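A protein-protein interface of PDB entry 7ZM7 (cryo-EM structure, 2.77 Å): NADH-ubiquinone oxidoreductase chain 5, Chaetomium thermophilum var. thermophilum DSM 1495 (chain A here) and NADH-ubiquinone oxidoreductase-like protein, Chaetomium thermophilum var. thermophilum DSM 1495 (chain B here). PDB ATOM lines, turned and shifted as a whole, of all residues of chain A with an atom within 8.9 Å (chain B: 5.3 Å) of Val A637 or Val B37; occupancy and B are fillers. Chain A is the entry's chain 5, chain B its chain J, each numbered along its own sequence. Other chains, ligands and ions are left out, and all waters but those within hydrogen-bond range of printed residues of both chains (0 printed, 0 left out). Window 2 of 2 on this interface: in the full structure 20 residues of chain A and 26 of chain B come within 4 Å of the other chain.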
ATOM      1  N   LEU A 623      24.483 -30.330 -24.245  1.00  0.00           N
ATOM      2  CA  LEU A 623      24.137 -29.542 -23.074  1.00  0.00           C
ATOM      3  C   LEU A 623      23.525 -28.198 -23.439  1.00  0.00           C
ATOM      4  O   LEU A 623      22.722 -27.666 -22.671  1.00  0.00           O
ATOM      5  CB  LEU A 623      25.383 -29.332 -22.218  1.00  0.00           C
ATOM      6  CG  LEU A 623      25.836 -30.553 -21.431  1.00  0.00           C
ATOM      7  CD1 LEU A 623      27.292 -30.433 -21.038  1.00  0.00           C
ATOM      8  CD2 LEU A 623      24.975 -30.705 -20.205  1.00  0.00           C
ATOM      9  N   THR A 630      18.049 -23.324 -17.613  1.00  0.00           N
ATOM     10  CA  THR A 630      19.123 -24.338 -17.448  1.00  0.00           C
ATOM     11  C   THR A 630      20.496 -23.651 -17.419  1.00  0.00           C
ATOM     12  O   THR A 630      21.387 -24.147 -16.708  1.00  0.00           O
ATOM     13  CB  THR A 630      18.984 -25.475 -18.466  1.00  0.00           C
ATOM     14  OG1 THR A 630      19.515 -25.077 -19.728  1.00  0.00           O
ATOM     15  CG2 THR A 630      17.556 -25.952 -18.618  1.00  0.00           C
ATOM     16  N   TYR A 631      20.660 -22.569 -18.175  1.00  0.00           N
ATOM     17  CA  TYR A 631      21.947 -21.830 -18.200  1.00  0.00           C
ATOM     18  C   TYR A 631      22.243 -21.237 -16.829  1.00  0.00           C
ATOM     19  O   TYR A 631      23.401 -21.272 -16.408  1.00  0.00           O
ATOM     20  CB  TYR A 631      21.959 -20.786 -19.316  1.00  0.00           C
ATOM     21  CG  TYR A 631      22.127 -21.351 -20.704  1.00  0.00           C
ATOM     22  CD1 TYR A 631      22.396 -22.695 -20.905  1.00  0.00           C
ATOM     23  CD2 TYR A 631      22.025 -20.541 -21.819  1.00  0.00           C
ATOM     24  CE1 TYR A 631      22.548 -23.221 -22.177  1.00  0.00           C
ATOM     25  CE2 TYR A 631      22.176 -21.046 -23.098  1.00  0.00           C
ATOM     26  CZ  TYR A 631      22.441 -22.391 -23.278  1.00  0.00           C
ATOM     27  OH  TYR A 631      22.593 -22.891 -24.538  1.00  0.00           O
ATOM     28  N   ALA A 632      21.228 -20.709 -16.166  1.00  0.00           N
ATOM     29  CA  ALA A 632      21.403 -20.076 -14.846  1.00  0.00           C
ATOM     30  C   ALA A 632      21.914 -21.104 -13.842  1.00  0.00           C
ATOM     31  O   ALA A 632      22.818 -20.767 -13.054  1.00  0.00           O
ATOM     32  CB  ALA A 632      20.065 -19.566 -14.428  1.00  0.00           C
ATOM     33  N   LEU A 633      21.352 -22.312 -13.880  1.00  0.00           N
ATOM     34  CA  LEU A 633      21.759 -23.385 -12.954  1.00  0.00           C
ATOM     35  C   LEU A 633      23.220 -23.713 -13.241  1.00  0.00           C
ATOM     36  O   LEU A 633      23.974 -23.863 -12.283  1.00  0.00           O
ATOM     37  CB  LEU A 633      20.830 -24.575 -13.199  1.00  0.00           C
ATOM     38  CG  LEU A 633      20.908 -25.702 -12.173  1.00  0.00           C
ATOM     39  CD1 LEU A 633      20.749 -25.158 -10.763  1.00  0.00           C
ATOM     40  CD2 LEU A 633      19.857 -26.762 -12.459  1.00  0.00           C
ATOM     41  N   TYR A 634      23.607 -23.756 -14.517  1.00  0.00           N
ATOM     42  CA  TYR A 634      24.999 -24.113 -14.888  1.00  0.00           C
ATOM     43  C   TYR A 634      25.976 -23.072 -14.333  1.00  0.00           C
ATOM     44  O   TYR A 634      27.054 -23.465 -13.869  1.00  0.00           O
ATOM     45  CB  TYR A 634      25.178 -24.208 -16.406  1.00  0.00           C
ATOM     46  CG  TYR A 634      24.495 -25.338 -17.130  1.00  0.00           C
ATOM     47  CD1 TYR A 634      24.038 -26.462 -16.464  1.00  0.00           C
ATOM     48  CD2 TYR A 634      24.327 -25.283 -18.503  1.00  0.00           C
ATOM     49  CE1 TYR A 634      23.421 -27.496 -17.147  1.00  0.00           C
ATOM     50  CE2 TYR A 634      23.716 -26.310 -19.200  1.00  0.00           C
ATOM     51  CZ  TYR A 634      23.258 -27.419 -18.517  1.00  0.00           C
ATOM     52  OH  TYR A 634      22.645 -28.430 -19.196  1.00  0.00           O
ATOM     53  N   ILE A 635      25.622 -21.793 -14.400  1.00  0.00           N
ATOM     54  CA  ILE A 635      26.492 -20.700 -13.865  1.00  0.00           C
ATOM     55  C   ILE A 635      26.649 -20.848 -12.349  1.00  0.00           C
ATOM     56  O   ILE A 635      27.769 -20.650 -11.864  1.00  0.00           O
ATOM     57  CB  ILE A 635      25.932 -19.316 -14.248  1.00  0.00           C
ATOM     58  CG1 ILE A 635      26.047 -19.055 -15.750  1.00  0.00           C
ATOM     59  CG2 ILE A 635      26.582 -18.204 -13.438  1.00  0.00           C
ATOM     60  CD1 ILE A 635      25.161 -17.939 -16.235  1.00  0.00           C
ATOM     61  N   LEU A 636      25.571 -21.196 -11.639  1.00  0.00           N
ATOM     62  CA  LEU A 636      25.608 -21.378 -10.167  1.00  0.00           C
ATOM     63  C   LEU A 636      26.393 -22.646  -9.865  1.00  0.00           C
ATOM     64  O   LEU A 636      27.165 -22.646  -8.899  1.00  0.00           O
ATOM     65  CB  LEU A 636      24.162 -21.465  -9.686  1.00  0.00           C
ATOM     66  CG  LEU A 636      23.898 -21.807  -8.225  1.00  0.00           C
ATOM     67  CD1 LEU A 636      22.622 -21.120  -7.787  1.00  0.00           C
ATOM     68  CD2 LEU A 636      23.758 -23.311  -8.031  1.00  0.00           C
ATOM     69  N   VAL A 637      26.211 -23.683 -10.679  1.00  0.00           N
ATOM     70  CA  VAL A 637      27.016 -24.877 -10.464  1.00  0.00           C
ATOM     71  C   VAL A 637      28.485 -24.547 -10.632  1.00  0.00           C
ATOM     72  O   VAL A 637      29.317 -24.903  -9.794  1.00  0.00           O
ATOM     73  CB  VAL A 637      26.579 -26.004 -11.416  1.00  0.00           C
ATOM     74  CG1 VAL A 637      27.581 -27.144 -11.379  1.00  0.00           C
ATOM     75  CG2 VAL A 637      25.204 -26.497 -11.037  1.00  0.00           C
ATOM     76  N   GLY A 638      28.821 -23.831 -11.703  1.00  0.00           N
ATOM     77  CA  GLY A 638      30.197 -23.420 -11.915  1.00  0.00           C
ATOM     78  C   GLY A 638      30.689 -22.429 -10.884  1.00  0.00           C
ATOM     79  O   GLY A 638      31.892 -22.293 -10.677  1.00  0.00           O
ATOM     80  N   PHE A 639      29.774 -21.710 -10.243  1.00  0.00           N
ATOM     81  CA  PHE A 639      30.149 -20.854  -9.122  1.00  0.00           C
ATOM     82  C   PHE A 639      30.472 -21.661  -7.871  1.00  0.00           C
ATOM     83  O   PHE A 639      31.448 -21.366  -7.183  1.00  0.00           O
ATOM     84  CB  PHE A 639      29.052 -19.831  -8.868  1.00  0.00           C
ATOM     85  CG  PHE A 639      29.431 -18.756  -7.894  1.00  0.00           C
ATOM     86  CD1 PHE A 639      30.410 -17.831  -8.202  1.00  0.00           C
ATOM     87  CD2 PHE A 639      28.871 -18.726  -6.625  1.00  0.00           C
ATOM     88  CE1 PHE A 639      30.771 -16.848  -7.295  1.00  0.00           C
ATOM     89  CE2 PHE A 639      29.218 -17.755  -5.725  1.00  0.00           C
ATOM     90  CZ  PHE A 639      30.172 -16.818  -6.051  1.00  0.00           C
ATOM     91  N   ILE A 640      29.681 -22.685  -7.565  1.00  0.00           N
ATOM     92  CA  ILE A 640      29.915 -23.457  -6.350  1.00  0.00           C
ATOM     93  C   ILE A 640      31.261 -24.163  -6.410  1.00  0.00           C
ATOM     94  O   ILE A 640      32.018 -24.177  -5.433  1.00  0.00           O
ATOM     95  CB  ILE A 640      28.768 -24.453  -6.123  1.00  0.00           C
ATOM     96  CG1 ILE A 640      27.442 -23.712  -5.999  1.00  0.00           C
ATOM     97  CG2 ILE A 640      29.045 -25.325  -4.909  1.00  0.00           C
ATOM     98  CD1 ILE A 640      27.393 -22.751  -4.842  1.00  0.00           C
ATOM     99  N   LEU A 641      31.583 -24.749  -7.558  1.00  0.00           N
ATOM    100  CA  LEU A 641      32.834 -25.479  -7.686  1.00  0.00           C
ATOM    101  C   LEU A 641      34.032 -24.559  -7.489  1.00  0.00           C
ATOM    102  O   LEU A 641      35.063 -24.980  -6.955  1.00  0.00           O
ATOM    103  CB  LEU A 641      32.879 -26.169  -9.046  1.00  0.00           C
ATOM    104  CG  LEU A 641      31.629 -27.002  -9.320  1.00  0.00           C
ATOM    105  CD1 LEU A 641      31.457 -27.288 -10.793  1.00  0.00           C
ATOM    106  CD2 LEU A 641      31.696 -28.297  -8.534  1.00  0.00           C
ATOM    107  N   TYR A 642      33.924 -23.302  -7.926  1.00  0.00           N
ATOM    108  CA  TYR A 642      35.008 -22.354  -7.696  1.00  0.00           C
ATOM    109  C   TYR A 642      35.168 -22.044  -6.220  1.00  0.00           C
ATOM    110  O   TYR A 642      36.290 -21.950  -5.721  1.00  0.00           O
ATOM    111  CB  TYR A 642      34.772 -21.069  -8.483  1.00  0.00           C
ATOM    112  CG  TYR A 642      35.266 -21.145  -9.896  1.00  0.00           C
ATOM    113  CD1 TYR A 642      35.027 -22.257 -10.670  1.00  0.00           C
ATOM    114  CD2 TYR A 642      35.980 -20.115 -10.451  1.00  0.00           C
ATOM    115  CE1 TYR A 642      35.472 -22.324 -11.956  1.00  0.00           C
ATOM    116  CE2 TYR A 642      36.421 -20.172 -11.738  1.00  0.00           C
ATOM    117  CZ  TYR A 642      36.176 -21.272 -12.482  1.00  0.00           C
ATOM    118  OH  TYR A 642      36.634 -21.328 -13.771  1.00  0.00           O
ATOM    119  N   LEU A 643      34.058 -21.863  -5.515  1.00  0.00           N
ATOM    120  CA  LEU A 643      34.110 -21.610  -4.082  1.00  0.00           C
ATOM    121  C   LEU A 643      34.649 -22.809  -3.326  1.00  0.00           C
ATOM    122  O   LEU A 643      35.491 -22.660  -2.436  1.00  0.00           O
ATOM    123  CB  LEU A 643      32.726 -21.224  -3.571  1.00  0.00           C
ATOM    124  CG  LEU A 643      32.302 -19.765  -3.718  1.00  0.00           C
ATOM    125  CD1 LEU A 643      33.221 -18.928  -2.873  1.00  0.00           C
ATOM    126  CD2 LEU A 643      32.366 -19.284  -5.132  1.00  0.00           C
ATOM    127  N   ILE A 644      34.184 -24.007  -3.669  1.00  0.00           N
ATOM    128  CA  ILE A 644      34.720 -25.205  -3.041  1.00  0.00           C
ATOM    129  C   ILE A 644      36.208 -25.320  -3.300  1.00  0.00           C
ATOM    130  O   ILE A 644      36.998 -25.530  -2.375  1.00  0.00           O
ATOM    131  CB  ILE A 644      33.965 -26.452  -3.529  1.00  0.00           C
ATOM    132  CG1 ILE A 644      32.556 -26.478  -2.936  1.00  0.00           C
ATOM    133  CG2 ILE A 644      34.739 -27.701  -3.199  1.00  0.00           C
ATOM    134  CD1 ILE A 644      31.675 -27.531  -3.542  1.00  0.00           C
ATOM    135  N   LEU A 662      35.143 -36.106 -15.791  1.00  0.00           N
ATOM    136  CA  LEU A 662      34.041 -35.548 -16.561  1.00  0.00           C
ATOM    137  C   LEU A 662      34.205 -35.801 -18.053  1.00  0.00           C
ATOM    138  O   LEU A 662      33.255 -36.227 -18.719  1.00  0.00           O
ATOM    139  CB  LEU A 662      33.904 -34.056 -16.287  1.00  0.00           C
ATOM    140  CG  LEU A 662      33.560 -33.696 -14.847  1.00  0.00           C
ATOM    141  CD1 LEU A 662      33.568 -32.191 -14.650  1.00  0.00           C
ATOM    142  CD2 LEU A 662      32.211 -34.287 -14.455  1.00  0.00           C
ATOM    143  N   LEU B  33      26.849 -33.761  -5.981  1.00  0.00           N
ATOM    144  CA  LEU B  33      26.290 -32.499  -6.451  1.00  0.00           C
ATOM    145  C   LEU B  33      25.987 -32.553  -7.940  1.00  0.00           C
ATOM    146  O   LEU B  33      25.095 -31.845  -8.419  1.00  0.00           O
ATOM    147  CB  LEU B  33      27.250 -31.350  -6.137  1.00  0.00           C
ATOM    148  CG  LEU B  33      26.819 -29.892  -6.366  1.00  0.00           C
ATOM    149  CD1 LEU B  33      27.598 -29.004  -5.415  1.00  0.00           C
ATOM    150  CD2 LEU B  33      27.002 -29.396  -7.789  1.00  0.00           C
ATOM    151  N   PHE B  34      26.720 -33.377  -8.689  1.00  0.00           N
ATOM    152  CA  PHE B  34      26.436 -33.509 -10.113  1.00  0.00           C
ATOM    153  C   PHE B  34      25.139 -34.265 -10.346  1.00  0.00           C
ATOM    154  O   PHE B  34      24.332 -33.876 -11.194  1.00  0.00           O
ATOM    155  CB  PHE B  34      27.600 -34.188 -10.815  1.00  0.00           C
ATOM    156  CG  PHE B  34      28.634 -33.232 -11.301  1.00  0.00           C
ATOM    157  CD1 PHE B  34      28.295 -32.219 -12.177  1.00  0.00           C
ATOM    158  CD2 PHE B  34      29.939 -33.318 -10.857  1.00  0.00           C
ATOM    159  CE1 PHE B  34      29.242 -31.327 -12.621  1.00  0.00           C
ATOM    160  CE2 PHE B  34      30.889 -32.429 -11.295  1.00  0.00           C
ATOM    161  CZ  PHE B  34      30.542 -31.432 -12.179  1.00  0.00           C
ATOM    162  N   ALA B  35      24.909 -35.328  -9.581  1.00  0.00           N
ATOM    163  CA  ALA B  35      23.644 -36.038  -9.662  1.00  0.00           C
ATOM    164  C   ALA B  35      22.484 -35.147  -9.244  1.00  0.00           C
ATOM    165  O   ALA B  35      21.355 -35.324  -9.715  1.00  0.00           O
ATOM    166  CB  ALA B  35      23.700 -37.290  -8.794  1.00  0.00           C
ATOM    167  N   ALA B  36      22.735 -34.195  -8.344  1.00  0.00           N
ATOM    168  CA  ALA B  36      21.694 -33.245  -7.979  1.00  0.00           C
ATOM    169  C   ALA B  36      21.311 -32.370  -9.166  1.00  0.00           C
ATOM    170  O   ALA B  36      20.143 -32.010  -9.336  1.00  0.00           O
ATOM    171  CB  ALA B  36      22.158 -32.394  -6.806  1.00  0.00           C
ATOM    172  N   VAL B  37      22.291 -32.011  -9.990  1.00  0.00           N
ATOM    173  CA  VAL B  37      22.020 -31.256 -11.206  1.00  0.00           C
ATOM    174  C   VAL B  37      21.210 -32.096 -12.175  1.00  0.00           C
ATOM    175  O   VAL B  37      20.308 -31.594 -12.854  1.00  0.00           O
ATOM    176  CB  VAL B  37      23.347 -30.795 -11.830  1.00  0.00           C
ATOM    177  CG1 VAL B  37      23.105 -30.058 -13.126  1.00  0.00           C
ATOM    178  CG2 VAL B  37      24.113 -29.939 -10.845  1.00  0.00           C
ATOM    179  N   ARG B  38      21.533 -33.389 -12.265  1.00  0.00           N
ATOM    180  CA  ARG B  38      20.848 -34.284 -13.188  1.00  0.00           C
ATOM    181  C   ARG B  38      19.376 -34.418 -12.847  1.00  0.00           C
ATOM    182  O   ARG B  38      18.526 -34.450 -13.739  1.00  0.00           O
ATOM    183  CB  ARG B  38      21.522 -35.651 -13.179  1.00  0.00           C
ATOM    184  CG  ARG B  38      22.957 -35.687 -13.671  1.00  0.00           C
ATOM    185  CD  ARG B  38      23.000 -35.389 -15.151  1.00  0.00           C
ATOM    186  NE  ARG B  38      22.233 -36.380 -15.897  1.00  0.00           N
ATOM    187  CZ  ARG B  38      22.714 -37.544 -16.317  1.00  0.00           C
ATOM    188  NH1 ARG B  38      23.975 -37.871 -16.073  1.00  0.00           N
ATOM    189  NH2 ARG B  38      21.932 -38.379 -16.982  1.00  0.00           N
ATOM    190  N   THR B  39      19.059 -34.520 -11.561  1.00  0.00           N
ATOM    191  CA  THR B  39      17.674 -34.669 -11.150  1.00  0.00           C
ATOM    192  C   THR B  39      16.916 -33.363 -11.288  1.00  0.00           C
ATOM    193  O   THR B  39      15.751 -33.355 -11.699  1.00  0.00           O
ATOM    194  CB  THR B  39      17.608 -35.176  -9.714  1.00  0.00           C
ATOM    195  OG1 THR B  39      18.231 -34.227  -8.852  1.00  0.00           O
ATOM    196  CG2 THR B  39      18.325 -36.483  -9.589  1.00  0.00           C
ATOM    197  N   SER B  40      17.559 -32.249 -10.945  1.00  0.00           N
ATOM    198  CA  SER B  40      16.905 -30.958 -11.092  1.00  0.00           C
ATOM    199  C   SER B  40      16.559 -30.683 -12.545  1.00  0.00           C
ATOM    200  O   SER B  40      15.519 -30.082 -12.830  1.00  0.00           O
ATOM    201  CB  SER B  40      17.791 -29.858 -10.528  1.00  0.00           C
ATOM    202  OG  SER B  40      17.185 -28.598 -10.687  1.00  0.00           O
ATOM    203  N   LEU B  41      17.399 -31.131 -13.473  1.00  0.00           N
ATOM    204  CA  LEU B  41      17.144 -30.950 -14.893  1.00  0.00           C
ATOM    205  C   LEU B  41      16.402 -32.109 -15.529  1.00  0.00           C
ATOM    206  O   LEU B  41      16.204 -32.097 -16.744  1.00  0.00           O
ATOM    207  CB  LEU B  41      18.442 -30.703 -15.660  1.00  0.00           C
ATOM    208  CG  LEU B  41      19.124 -29.370 -15.383  1.00  0.00           C
ATOM    209  CD1 LEU B  41      20.437 -29.264 -16.131  1.00  0.00           C
ATOM    210  CD2 LEU B  41      18.191 -28.238 -15.740  1.00  0.00           C
ATOM    211  N   ALA B  42      15.985 -33.096 -14.749  1.00  0.00           N
ATOM    212  CA  ALA B  42      15.126 -34.142 -15.280  1.00  0.00           C
ATOM    213  C   ALA B  42      13.855 -33.532 -15.849  1.00  0.00           C
ATOM    214  O   ALA B  42      13.280 -32.608 -15.271  1.00  0.00           O
ATOM    215  CB  ALA B  42      14.786 -35.152 -14.188  1.00  0.00           C
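Printed residues of chain A that touch a printed residue of chain B: Thr A630, Leu A633, Tyr A634, Val A637, Ile A640 and Leu A662.
Hydrophobic or aromatic side chains of chain A within 4 Å of the printed part of chain B: Leu A633, Tyr A634, Val A637, Ile A640 and Leu A662.
Printed residues of chain B that touch a printed residue of chain A: Leu B33, Phe B34, Val B37, Ser B40 and Leu B41.
Hydrophobic or aromatic side chains of chain B that line the printed part of chain A: Leu B33, Phe B34, Val B37 and Leu B41.
Along chain B the printed residues that touch a printed residue of chain A span positions 33 to 41.
Among the printed residues, no Asp or Glu carboxylate lies within 4 Å of a Lys or Arg side-chain nitrogen of the other chain.
Ala A632 touches none of the printed residues of chain B.
Printed residues of chain B within 4 Å of Leu A633: Ser B40 and Leu B41.
Val A637 touches just one residue of chain B: Val B37.
Printed residues of chain B within 4 Å of Leu A662: Phe B34.
Val B37 touches one residue of chain A.
The nearest residue of chain A that does not touch Val B37 is Leu A633 (4.7 Å).
The nearest printed residue of chain A that does not touch Leu B41 is Leu A623 (6.3 Å).
Among the printed residues, pairs that only touch across the chains: Thr A630 with Leu B41, Leu A633 with Ser B40, Leu A633 with Leu B41, Tyr A634 with Leu B41, Val A637 with Val B37, Ile A640 with Leu B33 and Leu A662 with Phe B34.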
